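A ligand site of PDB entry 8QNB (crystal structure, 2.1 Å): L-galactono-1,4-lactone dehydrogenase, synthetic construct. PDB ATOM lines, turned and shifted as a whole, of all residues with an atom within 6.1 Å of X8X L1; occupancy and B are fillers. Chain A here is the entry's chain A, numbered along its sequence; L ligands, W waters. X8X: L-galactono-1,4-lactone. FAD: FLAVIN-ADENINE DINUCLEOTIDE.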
ATOM      1  N   PRO A  58      -3.182  24.824 -23.912  1.00  0.00           N
ATOM      2  CA  PRO A  58      -4.407  25.162 -24.643  1.00  0.00           C
ATOM      3  C   PRO A  58      -5.703  25.045 -23.827  1.00  0.00           C
ATOM      4  O   PRO A  58      -6.593  25.811 -24.071  1.00  0.00           O
ATOM      5  CB  PRO A  58      -4.374  24.159 -25.799  1.00  0.00           C
ATOM      6  CG  PRO A  58      -2.895  24.027 -26.077  1.00  0.00           C
ATOM      7  CD  PRO A  58      -2.258  23.994 -24.703  1.00  0.00           C
ATOM      8  N   SER A 114       7.175  21.569 -30.265  1.00  0.00           N
ATOM      9  CA  SER A 114       7.138  22.582 -31.351  1.00  0.00           C
ATOM     10  C   SER A 114       7.489  23.963 -30.796  1.00  0.00           C
ATOM     11  O   SER A 114       7.930  24.802 -31.610  1.00  0.00           O
ATOM     12  CB  SER A 114       5.821  22.567 -32.078  1.00  0.00           C
ATOM     13  OG  SER A 114       4.720  22.665 -31.188  1.00  0.00           O
ATOM     14  N   HIS A 129       5.705  15.817 -25.554  1.00  0.00           N
ATOM     15  CA  HIS A 129       6.416  14.919 -26.488  1.00  0.00           C
ATOM     16  C   HIS A 129       6.820  15.674 -27.743  1.00  0.00           C
ATOM     17  O   HIS A 129       6.201  16.718 -28.058  1.00  0.00           O
ATOM     18  CB  HIS A 129       5.526  13.712 -26.859  1.00  0.00           C
ATOM     19  CG  HIS A 129       4.403  14.122 -27.756  1.00  0.00           C
ATOM     20  ND1 HIS A 129       4.554  14.167 -29.127  1.00  0.00           N
ATOM     21  CD2 HIS A 129       3.164  14.578 -27.485  1.00  0.00           C
ATOM     22  CE1 HIS A 129       3.434  14.612 -29.663  1.00  0.00           C
ATOM     23  NE2 HIS A 129       2.572  14.870 -28.672  1.00  0.00           N
ATOM     24  N   PHE A 338       8.995  24.381 -34.579  1.00  0.00           N
ATOM     25  CA  PHE A 338       8.096  24.610 -35.743  1.00  0.00           C
ATOM     26  C   PHE A 338       7.300  25.904 -35.526  1.00  0.00           C
ATOM     27  O   PHE A 338       6.974  26.229 -34.383  1.00  0.00           O
ATOM     28  CB  PHE A 338       7.195  23.388 -35.938  1.00  0.00           C
ATOM     29  CG  PHE A 338       6.215  23.487 -37.071  1.00  0.00           C
ATOM     30  CD1 PHE A 338       6.633  23.497 -38.392  1.00  0.00           C
ATOM     31  CD2 PHE A 338       4.849  23.588 -36.811  1.00  0.00           C
ATOM     32  CE1 PHE A 338       5.724  23.604 -39.431  1.00  0.00           C
ATOM     33  CE2 PHE A 338       3.931  23.684 -37.855  1.00  0.00           C
ATOM     34  CZ  PHE A 338       4.366  23.684 -39.165  1.00  0.00           C
ATOM     35  N   ASP A 339       7.035  26.669 -36.593  1.00  0.00           N
ATOM     36  CA  ASP A 339       6.177  27.881 -36.537  1.00  0.00           C
ATOM     37  C   ASP A 339       4.714  27.402 -36.526  1.00  0.00           C
ATOM     38  O   ASP A 339       4.228  26.962 -37.582  1.00  0.00           O
ATOM     39  CB  ASP A 339       6.443  28.827 -37.703  1.00  0.00           C
ATOM     40  CG  ASP A 339       5.799  30.210 -37.598  1.00  0.00           C
ATOM     41  OD1 ASP A 339       4.729  30.356 -36.939  1.00  0.00           O
ATOM     42  OD2 ASP A 339       6.357  31.144 -38.220  1.00  0.00           O
ATOM     43  N   CYS A 340       4.054  27.471 -35.363  1.00  0.00           N
ATOM     44  CA  CYS A 340       2.713  26.877 -35.104  1.00  0.00           C
ATOM     45  C   CYS A 340       1.621  27.830 -35.614  1.00  0.00           C
ATOM     46  O   CYS A 340       0.450  27.408 -35.703  1.00  0.00           O
ATOM     47  CB  CYS A 340       2.521  26.553 -33.632  1.00  0.00           C
ATOM     48  SG  CYS A 340       3.827  25.477 -32.996  1.00  0.00           S
ATOM     49  N   GLY A 341       2.036  29.039 -36.008  1.00  0.00           N
ATOM     50  CA  GLY A 341       1.136  30.034 -36.610  1.00  0.00           C
ATOM     51  C   GLY A 341       0.407  30.843 -35.543  1.00  0.00           C
ATOM     52  O   GLY A 341       0.966  31.043 -34.440  1.00  0.00           O
ATOM     53  N   GLN A 344      -5.205  29.590 -31.975  1.00  0.00           N
ATOM     54  CA  GLN A 344      -5.760  28.341 -32.542  1.00  0.00           C
ATOM     55  C   GLN A 344      -6.450  27.534 -31.450  1.00  0.00           C
ATOM     56  O   GLN A 344      -6.103  27.723 -30.258  1.00  0.00           O
ATOM     57  CB  GLN A 344      -4.624  27.515 -33.134  1.00  0.00           C
ATOM     58  CG  GLN A 344      -3.450  27.397 -32.173  1.00  0.00           C
ATOM     59  CD  GLN A 344      -2.176  26.965 -32.843  1.00  0.00           C
ATOM     60  OE1 GLN A 344      -1.689  27.591 -33.798  1.00  0.00           O
ATOM     61  NE2 GLN A 344      -1.651  25.853 -32.363  1.00  0.00           N
ATOM     62  N   VAL A 346      -6.558  23.448 -30.677  1.00  0.00           N
ATOM     63  CA  VAL A 346      -5.861  22.178 -31.017  1.00  0.00           C
ATOM     64  C   VAL A 346      -6.489  21.021 -30.251  1.00  0.00           C
ATOM     65  O   VAL A 346      -6.934  21.214 -29.104  1.00  0.00           O
ATOM     66  CB  VAL A 346      -4.350  22.246 -30.758  1.00  0.00           C
ATOM     67  CG1 VAL A 346      -3.664  23.144 -31.784  1.00  0.00           C
ATOM     68  CG2 VAL A 346      -4.052  22.708 -29.344  1.00  0.00           C
ATOM     69  N   GLU A 348      -5.070  16.873 -29.723  1.00  0.00           N
ATOM     70  CA  GLU A 348      -4.031  15.875 -30.070  1.00  0.00           C
ATOM     71  C   GLU A 348      -4.294  14.588 -29.283  1.00  0.00           C
ATOM     72  O   GLU A 348      -4.389  14.643 -28.054  1.00  0.00           O
ATOM     73  CB  GLU A 348      -2.632  16.449 -29.791  1.00  0.00           C
ATOM     74  CG  GLU A 348      -1.539  15.751 -30.597  1.00  0.00           C
ATOM     75  CD  GLU A 348      -0.107  15.903 -30.082  1.00  0.00           C
ATOM     76  OE1 GLU A 348       0.053  16.351 -28.934  1.00  0.00           O
ATOM     77  OE2 GLU A 348       0.836  15.579 -30.845  1.00  0.00           O
ATOM     78  N   ALA A 383      -5.019  23.441 -42.436  1.00  0.00           N
ATOM     79  CA  ALA A 383      -3.792  22.636 -42.323  1.00  0.00           C
ATOM     80  C   ALA A 383      -2.883  23.307 -41.300  1.00  0.00           C
ATOM     81  O   ALA A 383      -2.990  24.507 -41.046  1.00  0.00           O
ATOM     82  CB  ALA A 383      -3.140  22.527 -43.681  1.00  0.00           C
ATOM     83  N   PRO A 384      -1.966  22.539 -40.686  1.00  0.00           N
ATOM     84  CA  PRO A 384      -1.849  21.105 -40.930  1.00  0.00           C
ATOM     85  C   PRO A 384      -2.549  20.231 -39.887  1.00  0.00           C
ATOM     86  O   PRO A 384      -2.659  20.644 -38.753  1.00  0.00           O
ATOM     87  CB  PRO A 384      -0.347  20.876 -40.794  1.00  0.00           C
ATOM     88  CG  PRO A 384       0.099  21.904 -39.763  1.00  0.00           C
ATOM     89  CD  PRO A 384      -0.911  23.026 -39.798  1.00  0.00           C
ATOM     90  N   GLU A 386      -1.167  17.508 -37.909  1.00  0.00           N
ATOM     91  CA  GLU A 386       0.218  17.128 -37.590  1.00  0.00           C
ATOM     92  C   GLU A 386       0.212  15.679 -37.084  1.00  0.00           C
ATOM     93  O   GLU A 386      -0.643  15.352 -36.264  1.00  0.00           O
ATOM     94  CB  GLU A 386       0.800  18.110 -36.588  1.00  0.00           C
ATOM     95  CG  GLU A 386       2.226  17.826 -36.190  1.00  0.00           C
ATOM     96  CD  GLU A 386       2.740  18.831 -35.174  1.00  0.00           C
ATOM     97  OE1 GLU A 386       3.817  19.443 -35.440  1.00  0.00           O
ATOM     98  OE2 GLU A 386       2.073  18.987 -34.117  1.00  0.00           O
ATOM     99  N   ARG A 388       2.822  12.764 -35.497  1.00  0.00           N
ATOM    100  CA  ARG A 388       4.147  12.481 -34.917  1.00  0.00           C
ATOM    101  C   ARG A 388       4.118  11.076 -34.305  1.00  0.00           C
ATOM    102  O   ARG A 388       3.051  10.409 -34.367  1.00  0.00           O
ATOM    103  CB  ARG A 388       4.441  13.616 -33.940  1.00  0.00           C
ATOM    104  CG  ARG A 388       4.609  14.944 -34.662  1.00  0.00           C
ATOM    105  CD  ARG A 388       5.024  16.010 -33.668  1.00  0.00           C
ATOM    106  NE  ARG A 388       3.853  16.391 -32.891  1.00  0.00           N
ATOM    107  CZ  ARG A 388       3.837  17.332 -31.948  1.00  0.00           C
ATOM    108  NH1 ARG A 388       4.940  17.969 -31.612  1.00  0.00           N
ATOM    109  NH2 ARG A 388       2.693  17.615 -31.337  1.00  0.00           N
ATOM    110  N   ILE A 415      -6.660  21.049 -35.879  1.00  0.00           N
ATOM    111  CA  ILE A 415      -6.413  22.507 -35.699  1.00  0.00           C
ATOM    112  C   ILE A 415      -7.500  23.279 -36.450  1.00  0.00           C
ATOM    113  O   ILE A 415      -7.916  22.850 -37.564  1.00  0.00           O
ATOM    114  CB  ILE A 415      -4.997  22.910 -36.185  1.00  0.00           C
ATOM    115  CG1 ILE A 415      -4.654  24.351 -35.780  1.00  0.00           C
ATOM    116  CG2 ILE A 415      -4.847  22.698 -37.688  1.00  0.00           C
ATOM    117  CD1 ILE A 415      -3.170  24.591 -35.543  1.00  0.00           C
ATOM    118  N   TYR A 417      -7.760  27.687 -36.729  1.00  0.00           N
ATOM    119  CA  TYR A 417      -7.122  28.978 -36.411  1.00  0.00           C
ATOM    120  C   TYR A 417      -8.217  29.945 -35.972  1.00  0.00           C
ATOM    121  O   TYR A 417      -9.373  29.758 -36.395  1.00  0.00           O
ATOM    122  CB  TYR A 417      -6.299  29.449 -37.621  1.00  0.00           C
ATOM    123  CG  TYR A 417      -5.190  28.495 -37.976  1.00  0.00           C
ATOM    124  CD1 TYR A 417      -3.949  28.599 -37.376  1.00  0.00           C
ATOM    125  CD2 TYR A 417      -5.374  27.469 -38.883  1.00  0.00           C
ATOM    126  CE1 TYR A 417      -2.924  27.712 -37.676  1.00  0.00           C
ATOM    127  CE2 TYR A 417      -4.358  26.572 -39.188  1.00  0.00           C
ATOM    128  CZ  TYR A 417      -3.128  26.687 -38.571  1.00  0.00           C
ATOM    129  OH  TYR A 417      -2.084  25.850 -38.861  1.00  0.00           O
ATOM    130  N   HIS A 453      -4.039  14.271 -25.173  1.00  0.00           N
ATOM    131  CA  HIS A 453      -3.007  15.132 -24.545  1.00  0.00           C
ATOM    132  C   HIS A 453      -3.658  15.885 -23.393  1.00  0.00           C
ATOM    133  O   HIS A 453      -4.716  16.548 -23.623  1.00  0.00           O
ATOM    134  CB  HIS A 453      -2.445  16.091 -25.609  1.00  0.00           C
ATOM    135  CG  HIS A 453      -1.121  16.651 -25.255  1.00  0.00           C
ATOM    136  ND1 HIS A 453      -0.948  17.515 -24.188  1.00  0.00           N
ATOM    137  CD2 HIS A 453       0.088  16.490 -25.837  1.00  0.00           C
ATOM    138  CE1 HIS A 453       0.326  17.860 -24.129  1.00  0.00           C
ATOM    139  NE2 HIS A 453       0.985  17.247 -25.137  1.00  0.00           N
ATOM    140  N   LYS A 456      -4.616  19.552 -23.764  1.00  0.00           N
ATOM    141  CA  LYS A 456      -5.523  19.865 -24.896  1.00  0.00           C
ATOM    142  C   LYS A 456      -6.936  19.337 -24.622  1.00  0.00           C
ATOM    143  O   LYS A 456      -7.865  19.790 -25.301  1.00  0.00           O
ATOM    144  CB  LYS A 456      -4.879  19.349 -26.182  1.00  0.00           C
ATOM    145  CG  LYS A 456      -3.501  19.961 -26.441  1.00  0.00           C
ATOM    146  CD  LYS A 456      -2.806  19.503 -27.709  1.00  0.00           C
ATOM    147  CE  LYS A 456      -1.286  19.594 -27.618  1.00  0.00           C
ATOM    148  NZ  LYS A 456      -0.659  19.205 -28.900  1.00  0.00           N
HETATM  149  O1  X8X L   1      -0.291  22.383 -29.437  1.00  0.00           O
HETATM  150  C1  X8X L   1       0.321  22.276 -30.475  1.00  0.00           C
HETATM  151  O2  X8X L   1       0.058  23.065 -31.549  1.00  0.00           O
HETATM  152  C2  X8X L   1       1.054  22.807 -32.614  1.00  0.00           C
HETATM  153  C3  X8X L   1       0.416  23.104 -33.957  1.00  0.00           C
HETATM  154  O3  X8X L   1       0.173  24.462 -34.207  1.00  0.00           O
HETATM  155  C4  X8X L   1       0.871  22.289 -35.160  1.00  0.00           C
HETATM  156  O4  X8X L   1       0.276  22.739 -36.381  1.00  0.00           O
HETATM  157  C5  X8X L   1       1.507  21.370 -32.344  1.00  0.00           C
HETATM  158  O5  X8X L   1       2.834  21.117 -32.807  1.00  0.00           O
HETATM  159  C6  X8X L   1       1.497  21.363 -30.808  1.00  0.00           C
HETATM  160  O6  X8X L   1       1.380  20.075 -30.241  1.00  0.00           O
HETATM  161  PA  FAD L   2       1.222  25.023 -17.615  1.00  0.00           P
HETATM  162  O1A FAD L   2       0.136  25.054 -18.639  1.00  0.00           O
HETATM  163  O2A FAD L   2       1.547  26.262 -16.839  1.00  0.00           O
HETATM  164  O5B FAD L   2       0.936  23.844 -16.577  1.00  0.00           O
HETATM  165  C5B FAD L   2       0.811  22.500 -17.122  1.00  0.00           C
HETATM  166  C4B FAD L   2       0.589  21.506 -16.017  1.00  0.00           C
HETATM  167  O4B FAD L   2       1.762  21.417 -15.164  1.00  0.00           O
HETATM  168  C3B FAD L   2      -0.574  21.817 -15.053  1.00  0.00           C
HETATM  169  O3B FAD L   2      -1.122  20.588 -14.609  1.00  0.00           O
HETATM  170  C2B FAD L   2       0.119  22.501 -13.868  1.00  0.00           C
HETATM  171  O2B FAD L   2      -0.651  22.419 -12.696  1.00  0.00           O
HETATM  172  C1B FAD L   2       1.402  21.681 -13.819  1.00  0.00           C
HETATM  173  N9A FAD L   2       2.525  22.351 -13.240  1.00  0.00           N
HETATM  174  C8A FAD L   2       3.192  23.415 -13.769  1.00  0.00           C
HETATM  175  N7A FAD L   2       4.243  23.751 -13.069  1.00  0.00           N
HETATM  176  C5A FAD L   2       4.284  22.819 -12.041  1.00  0.00           C
HETATM  177  C6A FAD L   2       5.150  22.638 -10.964  1.00  0.00           C
HETATM  178  N6A FAD L   2       6.233  23.375 -10.775  1.00  0.00           N
HETATM  179  N1A FAD L   2       4.886  21.598 -10.117  1.00  0.00           N
HETATM  180  C2A FAD L   2       3.811  20.843 -10.345  1.00  0.00           C
HETATM  181  N3A FAD L   2       2.923  20.916 -11.338  1.00  0.00           N
HETATM  182  C4A FAD L   2       3.231  21.937 -12.151  1.00  0.00           C
HETATM  183  N1  FAD L   2       2.956  19.746 -26.070  1.00  0.00           N
HETATM  184  C2  FAD L   2       3.583  18.683 -26.588  1.00  0.00           C
HETATM  185  O2  FAD L   2       3.576  17.597 -26.007  1.00  0.00           O
HETATM  186  N3  FAD L   2       4.253  18.753 -27.797  1.00  0.00           N
HETATM  187  C4  FAD L   2       4.302  19.906 -28.531  1.00  0.00           C
HETATM  188  O4  FAD L   2       4.926  19.929 -29.578  1.00  0.00           O
HETATM  189  C4X FAD L   2       3.596  21.030 -28.046  1.00  0.00           C
HETATM  190  N5  FAD L   2       3.603  22.131 -28.750  1.00  0.00           N
HETATM  191  C5X FAD L   2       2.864  23.173 -28.286  1.00  0.00           C
HETATM  192  C6  FAD L   2       2.802  24.341 -29.069  1.00  0.00           C
HETATM  193  C7  FAD L   2       2.095  25.441 -28.670  1.00  0.00           C
HETATM  194  C7M FAD L   2       2.046  26.665 -29.556  1.00  0.00           C
HETATM  195  C8  FAD L   2       1.400  25.405 -27.427  1.00  0.00           C
HETATM  196  C8M FAD L   2       0.604  26.593 -26.965  1.00  0.00           C
HETATM  197  C9  FAD L   2       1.472  24.277 -26.639  1.00  0.00           C
HETATM  198  C9A FAD L   2       2.191  23.137 -27.041  1.00  0.00           C
HETATM  199  N10 FAD L   2       2.258  21.958 -26.303  1.00  0.00           N
HETATM  200  C10 FAD L   2       2.928  20.853 -26.780  1.00  0.00           C
HETATM  201  C1' FAD L   2       1.593  21.838 -24.994  1.00  0.00           C
HETATM  202  C2' FAD L   2       2.558  22.240 -23.899  1.00  0.00           C
HETATM  203  O2' FAD L   2       3.809  21.545 -23.965  1.00  0.00           O
HETATM  204  C3' FAD L   2       1.910  21.996 -22.544  1.00  0.00           C
HETATM  205  O3' FAD L   2       0.733  22.769 -22.516  1.00  0.00           O
HETATM  206  C4' FAD L   2       2.771  22.360 -21.340  1.00  0.00           C
HETATM  207  O4' FAD L   2       2.148  21.797 -20.180  1.00  0.00           O
HETATM  208  C5' FAD L   2       2.886  23.847 -21.182  1.00  0.00           C
HETATM  209  O5' FAD L   2       3.924  24.138 -20.211  1.00  0.00           O
HETATM  210  P   FAD L   2       3.630  25.282 -19.120  1.00  0.00           P
HETATM  211  O1P FAD L   2       4.895  25.630 -18.401  1.00  0.00           O
HETATM  212  O2P FAD L   2       2.911  26.389 -19.811  1.00  0.00           O
HETATM  213  O3P FAD L   2       2.612  24.493 -18.188  1.00  0.00           O
HETATM  214  O   HOH W   1       0.135  25.271 -37.139  1.00  0.00           O
HETATM  215  O   HOH W   2      -1.707  25.264 -29.598  1.00  0.00           O
HETATM  216  O   HOH W   3      -1.914  20.860 -36.164  1.00  0.00           O
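Val 346 touches X8X L1. CG of Pro 384 touches O4 of X8X L1, at 3.5 Å. Ile 415 touches X8X L1. Hydrophobic or aromatic side chains that line X8X L1: Val 346, Pro 384 and Ile 415. The nearest printed residue that does not touch X8X L1 is Phe 338 (4.1 Å).
The side-chain carboxylate of Glu 348 lies within salt-bridge range of the side-chain amino group of Lys 456 (2.9 Å). The side-chain carboxylate of Glu 386 lies within salt-bridge range of the guanidinium group of Arg 388. SG of Cys 340 sits at hydrogen-bond distance from OG of Ser 114. O of Ser 114 is in hydrogen-bond range of N of Phe 338. The backbone carbonyl oxygen of Cys 340 sits close to the side-chain amide oxygen of Gln 344 (2.9 Å). The guanidinium group (NH2) of Arg 388 lies within salt-bridge range of the side-chain carboxylate (OE2) of Glu 348 (2.8 Å). The side-chain sulfur (SG) of Cys 340 sits at hydrogen-bond distance from the backbone carbonyl oxygen (O) of Phe 338 (3.5 Å).
O6 of X8X L1 is in hydrogen-bond range of NZ of Lys 456 (2.6 Å). O5 of X8X L1 is in hydrogen-bond range of OE2 of Glu 386, 2.6 Å away. An oxygen (O5) of X8X L1 lies within hydrogen-bond range of the side-chain hydroxyl (OG) of Ser 114 (2.9 Å). O3 of X8X L1 is in hydrogen-bond range of NE2 of Gln 344, at 2.9 Å. NH2 of Arg 388 is in hydrogen-bond range of O6 of X8X L1 (3.0 Å). O3 of X8X L1 sits close to O of Cys 340 (3.3 Å). An oxygen (O4) of FAD L2 lies within hydrogen-bond range of the backbone NH of Ser 114 (2.9 Å). A nitrogen (N5) of FAD L2 sits at hydrogen-bond distance from the side-chain hydroxyl (OG) of Ser 114 (2.7 Å). NH1 of Arg 388 is in hydrogen-bond range of O4 of FAD L2, at 2.8 Å. The backbone NH (N) of His 129 is in hydrogen-bond range of an oxygen (O2) of FAD L2. N3 of FAD L2 is in hydrogen-bond range of O of His 129 (2.8 Å). An oxygen (O2) of FAD L2 is in hydrogen-bond range of a ring nitrogen (NE2) of His 453 (2.8 Å).
Water W1 lies within hydrogen-bond range of O of Cys 340 (2.6 Å), O4 of X8X L1 (2.6 Å) and OH of Tyr 417 (2.9 Å). Water W3 lies within hydrogen-bond range of O of Pro 384 (2.7 Å) and O4 of X8X L1 (2.9 Å). Water W2 lies within hydrogen-bond range of the side-chain amide nitrogen (NE2) of Gln 344 (2.8 Å) and an oxygen (O1) of X8X L1 (3.2 Å).
An oxygen (O6) of X8X L1 sits close to a nitrogen (N5) of FAD L2 (3.4 Å).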
